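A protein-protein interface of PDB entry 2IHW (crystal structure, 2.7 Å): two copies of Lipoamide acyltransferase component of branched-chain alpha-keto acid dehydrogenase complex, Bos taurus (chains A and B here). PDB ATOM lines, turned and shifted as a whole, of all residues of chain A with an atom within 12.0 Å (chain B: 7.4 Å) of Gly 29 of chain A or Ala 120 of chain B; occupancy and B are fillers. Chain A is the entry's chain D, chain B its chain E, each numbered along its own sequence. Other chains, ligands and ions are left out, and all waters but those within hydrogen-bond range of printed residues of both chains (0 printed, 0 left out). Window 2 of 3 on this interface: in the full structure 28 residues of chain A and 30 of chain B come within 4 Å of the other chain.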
ATOM      1  N   GLY A  29     -11.220 -12.505   8.136  1.00  0.00           N
ATOM      2  CA  GLY A  29     -12.688 -12.788   8.069  1.00  0.00           C
ATOM      3  C   GLY A  29     -13.004 -14.124   8.712  1.00  0.00           C
ATOM      4  O   GLY A  29     -13.899 -14.236   9.543  1.00  0.00           O
ATOM      5  N   LYS A  30     -12.263 -15.140   8.299  1.00  0.00           N
ATOM      6  CA  LYS A  30     -12.199 -16.405   9.012  1.00  0.00           C
ATOM      7  C   LYS A  30     -10.718 -16.823   8.987  1.00  0.00           C
ATOM      8  O   LYS A  30      -9.815 -16.067   8.535  1.00  0.00           O
ATOM      9  CB  LYS A  30     -13.072 -17.454   8.294  1.00  0.00           C
ATOM     10  CG  LYS A  30     -14.081 -18.244   9.160  1.00  0.00           C
ATOM     11  CD  LYS A  30     -15.192 -18.847   8.254  1.00  0.00           C
ATOM     12  CE  LYS A  30     -16.430 -19.421   9.034  1.00  0.00           C
ATOM     13  NZ  LYS A  30     -17.534 -19.935   8.011  1.00  0.00           N
ATOM     14  N   ASP A  31     -10.457 -18.032   9.453  1.00  0.00           N
ATOM     15  CA  ASP A  31      -9.122 -18.610   9.311  1.00  0.00           C
ATOM     16  C   ASP A  31      -8.921 -19.225   7.904  1.00  0.00           C
ATOM     17  O   ASP A  31      -9.686 -20.103   7.483  1.00  0.00           O
ATOM     18  CB  ASP A  31      -8.866 -19.621  10.442  1.00  0.00           C
ATOM     19  CG  ASP A  31      -8.889 -18.969  11.849  1.00  0.00           C
ATOM     20  OD1 ASP A  31      -9.043 -17.719  11.963  1.00  0.00           O
ATOM     21  OD2 ASP A  31      -8.746 -19.713  12.850  1.00  0.00           O
ATOM     22  N   ARG A  32      -7.918 -18.735   7.177  1.00  0.00           N
ATOM     23  CA  ARG A  32      -7.573 -19.290   5.872  1.00  0.00           C
ATOM     24  C   ARG A  32      -6.493 -20.412   6.027  1.00  0.00           C
ATOM     25  O   ARG A  32      -5.415 -20.169   6.584  1.00  0.00           O
ATOM     26  CB  ARG A  32      -7.116 -18.145   4.954  1.00  0.00           C
ATOM     27  CG  ARG A  32      -7.123 -18.430   3.449  1.00  0.00           C
ATOM     28  CD  ARG A  32      -6.444 -17.301   2.629  1.00  0.00           C
ATOM     29  NE  ARG A  32      -4.985 -17.220   2.817  1.00  0.00           N
ATOM     30  CZ  ARG A  32      -4.256 -16.089   2.747  1.00  0.00           C
ATOM     31  NH1 ARG A  32      -4.851 -14.923   2.493  1.00  0.00           N
ATOM     32  NH2 ARG A  32      -2.933 -16.113   2.937  1.00  0.00           N
ATOM     33  N   THR A  33      -6.796 -21.639   5.576  1.00  0.00           N
ATOM     34  CA  THR A  33      -5.808 -22.740   5.559  1.00  0.00           C
ATOM     35  C   THR A  33      -5.234 -22.983   4.162  1.00  0.00           C
ATOM     36  O   THR A  33      -5.966 -23.030   3.162  1.00  0.00           O
ATOM     37  CB  THR A  33      -6.343 -24.063   6.173  1.00  0.00           C
ATOM     38  OG1 THR A  33      -6.479 -23.904   7.582  1.00  0.00           O
ATOM     39  CG2 THR A  33      -5.373 -25.209   5.943  1.00  0.00           C
ATOM     40  N   GLU A  34      -3.926 -23.173   4.104  1.00  0.00           N
ATOM     41  CA  GLU A  34      -3.257 -23.068   2.839  1.00  0.00           C
ATOM     42  C   GLU A  34      -1.933 -23.846   2.831  1.00  0.00           C
ATOM     43  O   GLU A  34      -1.075 -23.619   3.681  1.00  0.00           O
ATOM     44  CB  GLU A  34      -3.066 -21.575   2.571  1.00  0.00           C
ATOM     45  CG  GLU A  34      -2.361 -21.175   1.301  1.00  0.00           C
ATOM     46  CD  GLU A  34      -1.806 -19.749   1.385  1.00  0.00           C
ATOM     47  OE1 GLU A  34      -0.553 -19.570   1.478  1.00  0.00           O
ATOM     48  OE2 GLU A  34      -2.625 -18.802   1.371  1.00  0.00           O
ATOM     49  N   LEU B 100      -1.475  -7.098  12.019  1.00  0.00           N
ATOM     50  CA  LEU B 100      -2.209  -6.797  10.748  1.00  0.00           C
ATOM     51  C   LEU B 100      -1.257  -6.717   9.527  1.00  0.00           C
ATOM     52  O   LEU B 100      -1.509  -7.333   8.515  1.00  0.00           O
ATOM     53  CB  LEU B 100      -3.056  -5.531  10.801  1.00  0.00           C
ATOM     54  CG  LEU B 100      -4.251  -5.492  11.749  1.00  0.00           C
ATOM     55  CD1 LEU B 100      -4.991  -4.148  11.659  1.00  0.00           C
ATOM     56  CD2 LEU B 100      -5.181  -6.674  11.494  1.00  0.00           C
ATOM     57  N   ASN B 106       0.719 -14.599  13.166  1.00  0.00           N
ATOM     58  CA  ASN B 106      -0.490 -14.940  13.927  1.00  0.00           C
ATOM     59  C   ASN B 106      -1.144 -16.175  13.331  1.00  0.00           C
ATOM     60  O   ASN B 106      -2.345 -16.237  13.173  1.00  0.00           O
ATOM     61  CB  ASN B 106      -1.496 -13.789  13.880  1.00  0.00           C
ATOM     62  CG  ASN B 106      -2.561 -13.932  14.939  1.00  0.00           C
ATOM     63  OD1 ASN B 106      -2.249 -13.819  16.127  1.00  0.00           O
ATOM     64  ND2 ASN B 106      -3.816 -14.237  14.539  1.00  0.00           N
ATOM     65  N   THR B 117      -2.323 -22.095   8.640  1.00  0.00           N
ATOM     66  CA  THR B 117      -3.616 -21.515   8.863  1.00  0.00           C
ATOM     67  C   THR B 117      -3.421 -20.114   9.415  1.00  0.00           C
ATOM     68  O   THR B 117      -2.872 -19.939  10.515  1.00  0.00           O
ATOM     69  CB  THR B 117      -4.389 -22.346   9.909  1.00  0.00           C
ATOM     70  OG1 THR B 117      -4.456 -23.701   9.466  1.00  0.00           O
ATOM     71  CG2 THR B 117      -5.800 -21.784  10.169  1.00  0.00           C
ATOM     72  N   TYR B 118      -3.871 -19.122   8.654  1.00  0.00           N
ATOM     73  CA  TYR B 118      -3.844 -17.734   9.073  1.00  0.00           C
ATOM     74  C   TYR B 118      -5.089 -17.433   9.920  1.00  0.00           C
ATOM     75  O   TYR B 118      -6.226 -17.670   9.475  1.00  0.00           O
ATOM     76  CB  TYR B 118      -3.814 -16.818   7.837  1.00  0.00           C
ATOM     77  CG  TYR B 118      -2.522 -16.941   7.035  1.00  0.00           C
ATOM     78  CD1 TYR B 118      -2.432 -17.825   5.948  1.00  0.00           C
ATOM     79  CD2 TYR B 118      -1.396 -16.179   7.365  1.00  0.00           C
ATOM     80  CE1 TYR B 118      -1.276 -17.947   5.230  1.00  0.00           C
ATOM     81  CE2 TYR B 118      -0.217 -16.307   6.658  1.00  0.00           C
ATOM     82  CZ  TYR B 118      -0.160 -17.197   5.601  1.00  0.00           C
ATOM     83  OH  TYR B 118       1.026 -17.351   4.904  1.00  0.00           O
ATOM     84  N   LYS B 119      -4.884 -16.900  11.127  1.00  0.00           N
ATOM     85  CA  LYS B 119      -6.001 -16.606  12.024  1.00  0.00           C
ATOM     86  C   LYS B 119      -6.400 -15.145  11.952  1.00  0.00           C
ATOM     87  O   LYS B 119      -5.587 -14.268  12.199  1.00  0.00           O
ATOM     88  CB  LYS B 119      -5.682 -16.948  13.489  1.00  0.00           C
ATOM     89  CG  LYS B 119      -4.967 -18.259  13.769  1.00  0.00           C
ATOM     90  CD  LYS B 119      -5.875 -19.462  13.691  1.00  0.00           C
ATOM     91  CE  LYS B 119      -5.096 -20.757  13.828  1.00  0.00           C
ATOM     92  NZ  LYS B 119      -4.879 -21.232  15.230  1.00  0.00           N
ATOM     93  N   ALA B 120      -7.675 -14.915  11.661  1.00  0.00           N
ATOM     94  CA  ALA B 120      -8.272 -13.591  11.642  1.00  0.00           C
ATOM     95  C   ALA B 120      -8.181 -12.867  13.004  1.00  0.00           C
ATOM     96  O   ALA B 120      -7.764 -11.710  13.041  1.00  0.00           O
ATOM     97  CB  ALA B 120      -9.717 -13.698  11.177  1.00  0.00           C
ATOM     98  N   SER B 121      -8.541 -13.551  14.100  1.00  0.00           N
ATOM     99  CA  SER B 121      -8.450 -13.026  15.460  1.00  0.00           C
ATOM    100  C   SER B 121      -7.037 -12.864  16.075  1.00  0.00           C
ATOM    101  O   SER B 121      -6.140 -13.705  15.874  1.00  0.00           O
ATOM    102  CB  SER B 121      -9.195 -13.970  16.390  1.00  0.00           C
ATOM    103  OG  SER B 121     -10.573 -13.742  16.368  1.00  0.00           O
ATOM    104  N   HIS B 122      -6.858 -11.799  16.869  1.00  0.00           N
ATOM    105  CA  HIS B 122      -5.645 -11.647  17.686  1.00  0.00           C
ATOM    106  C   HIS B 122      -6.033 -11.974  19.111  1.00  0.00           C
ATOM    107  O   HIS B 122      -6.432 -11.094  19.886  1.00  0.00           O
ATOM    108  CB  HIS B 122      -5.048 -10.244  17.565  1.00  0.00           C
ATOM    109  CG  HIS B 122      -4.730  -9.847  16.151  1.00  0.00           C
ATOM    110  ND1 HIS B 122      -4.432  -8.549  15.783  1.00  0.00           N
ATOM    111  CD2 HIS B 122      -4.694 -10.572  15.004  1.00  0.00           C
ATOM    112  CE1 HIS B 122      -4.204  -8.496  14.481  1.00  0.00           C
ATOM    113  NE2 HIS B 122      -4.375  -9.705  13.984  1.00  0.00           N
ATOM    114  N   ASN B 123      -5.984 -13.258  19.434  1.00  0.00           N
ATOM    115  CA  ASN B 123      -6.249 -13.704  20.757  1.00  0.00           C
ATOM    116  C   ASN B 123      -4.915 -13.854  21.415  1.00  0.00           C
ATOM    117  O   ASN B 123      -4.303 -14.927  21.352  1.00  0.00           O
ATOM    118  CB  ASN B 123      -6.918 -15.033  20.707  1.00  0.00           C
ATOM    119  CG  ASN B 123      -8.195 -15.003  19.951  1.00  0.00           C
ATOM    120  OD1 ASN B 123      -8.710 -16.057  19.625  1.00  0.00           O
ATOM    121  ND2 ASN B 123      -8.719 -13.814  19.641  1.00  0.00           N
ATOM    122  N   ASN B 141      -9.542 -11.208  20.389  1.00  0.00           N
ATOM    123  CA  ASN B 141      -9.832 -10.136  19.462  1.00  0.00           C
ATOM    124  C   ASN B 141      -9.276  -8.757  19.829  1.00  0.00           C
ATOM    125  O   ASN B 141     -10.026  -7.750  19.814  1.00  0.00           O
ATOM    126  CB  ASN B 141     -11.345 -10.045  19.252  1.00  0.00           C
ATOM    127  CG  ASN B 141     -11.880 -11.225  18.460  1.00  0.00           C
ATOM    128  OD1 ASN B 141     -11.305 -11.598  17.412  1.00  0.00           O
ATOM    129  ND2 ASN B 141     -12.955 -11.840  18.950  1.00  0.00           N
ATOM    130  N   GLN B 143      -7.662  -6.888  18.178  1.00  0.00           N
ATOM    131  CA  GLN B 143      -7.765  -5.975  17.037  1.00  0.00           C
ATOM    132  C   GLN B 143      -9.084  -5.119  17.001  1.00  0.00           C
ATOM    133  O   GLN B 143      -9.154  -4.093  16.323  1.00  0.00           O
ATOM    134  CB  GLN B 143      -7.551  -6.740  15.733  1.00  0.00           C
ATOM    135  CG  GLN B 143      -8.754  -7.525  15.212  1.00  0.00           C
ATOM    136  CD  GLN B 143      -9.072  -8.774  16.045  1.00  0.00           C
ATOM    137  OE1 GLN B 143      -8.178  -9.389  16.618  1.00  0.00           O
ATOM    138  NE2 GLN B 143     -10.356  -9.162  16.091  1.00  0.00           N
ATOM    139  N   THR B 175      -3.675 -17.132  19.811  1.00  0.00           N
ATOM    140  CA  THR B 175      -2.968 -17.118  18.547  1.00  0.00           C
ATOM    141  C   THR B 175      -1.560 -16.543  18.600  1.00  0.00           C
ATOM    142  O   THR B 175      -0.867 -16.640  17.624  1.00  0.00           O
ATOM    143  CB  THR B 175      -3.733 -16.385  17.476  1.00  0.00           C
ATOM    144  OG1 THR B 175      -3.932 -15.038  17.893  1.00  0.00           O
ATOM    145  CG2 THR B 175      -5.056 -17.050  17.240  1.00  0.00           C
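The backbone carbonyl oxygen of Arg 32 of chain A is in hydrogen-bond range of the backbone NH of Tyr 118 of chain B, at 2.8 Å.
The side-chain hydroxyl (OG1) of Thr 33 of chain A lies within hydrogen-bond range of the side-chain hydroxyl (OG1) of Thr 117 of chain B, 2.8 Å away.
The side-chain carboxylate (OD1) of Asp 31 of chain A lies within hydrogen-bond range of the backbone NH (N) of Ala 120 of chain B.
The side-chain amide nitrogen (ND2) of Asn 106 of chain B is in hydrogen-bond range of the backbone carbonyl oxygen (O) of Lys 119 of chain B, at 2.9 Å.
NH2 of Arg 32 of chain A is in salt-bridge range of OE2 of Glu 34 of chain A (3.1 Å).
Among the printed residues, merely in contact across the chains: Asp 31 of chain A with Lys 119 of chain B (3.0 Å), Asp 31 of chain A with Tyr 118 of chain B (3.0 Å), Arg 32 of chain A with Thr 117 of chain B (3.2 Å), Lys 30 of chain A with Ala 120 of chain B (3.5 Å), Gly 29 of chain A with Ala 120 of chain B (3.6 Å) and Asp 31 of chain A with Thr 117 of chain B (3.8 Å).
Printed residues of chain B within 4 Å of Gly 29 of chain A: Ala 120 (3.6 Å).
Of the printed residues of chain B, Lys 30 of chain A touches Ala 120 (3.5 Å).
Of the printed residues of chain B, Asp 31 of chain A touches Thr 117, Tyr 118, Lys 119 and Ala 120.
Of the printed residues of chain A, Thr 117 of chain B touches Asp 31 (3.8 Å), Arg 32 (3.2 Å) and Thr 33 (2.8 Å).
Of the printed residues of chain A, Tyr 118 of chain B touches Asp 31 (3.0 Å) and Arg 32 (2.8 Å).
Of the printed residues of chain A, Lys 119 of chain B touches Asp 31 (3.0 Å).
Ala 120 of chain B touches three residues of chain A.
No residue of chain A comes within 4 Å of Ser 121 of chain B.
No residue of chain A comes within 4 Å of His 122 of chain B.
Of the 12 printed residues of chain B, 4 touch a printed residue of chain A.
Along chain B the printed residues that touch a printed residue of chain A span positions 117 to 120.
Of the 6 printed residues of chain A, 5 touch a printed residue of chain B.
Among the printed residues, 9 pairs touch across the chains.
Among the printed residues, no Asp or Glu carboxylate lies within 4 Å of a Lys or Arg side-chain nitrogen of the other chain.
No position is printed for both chains.
Of the 9 pairs that touch across the chains among the printed residues, none has its exchanged pair printed and touching as well.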
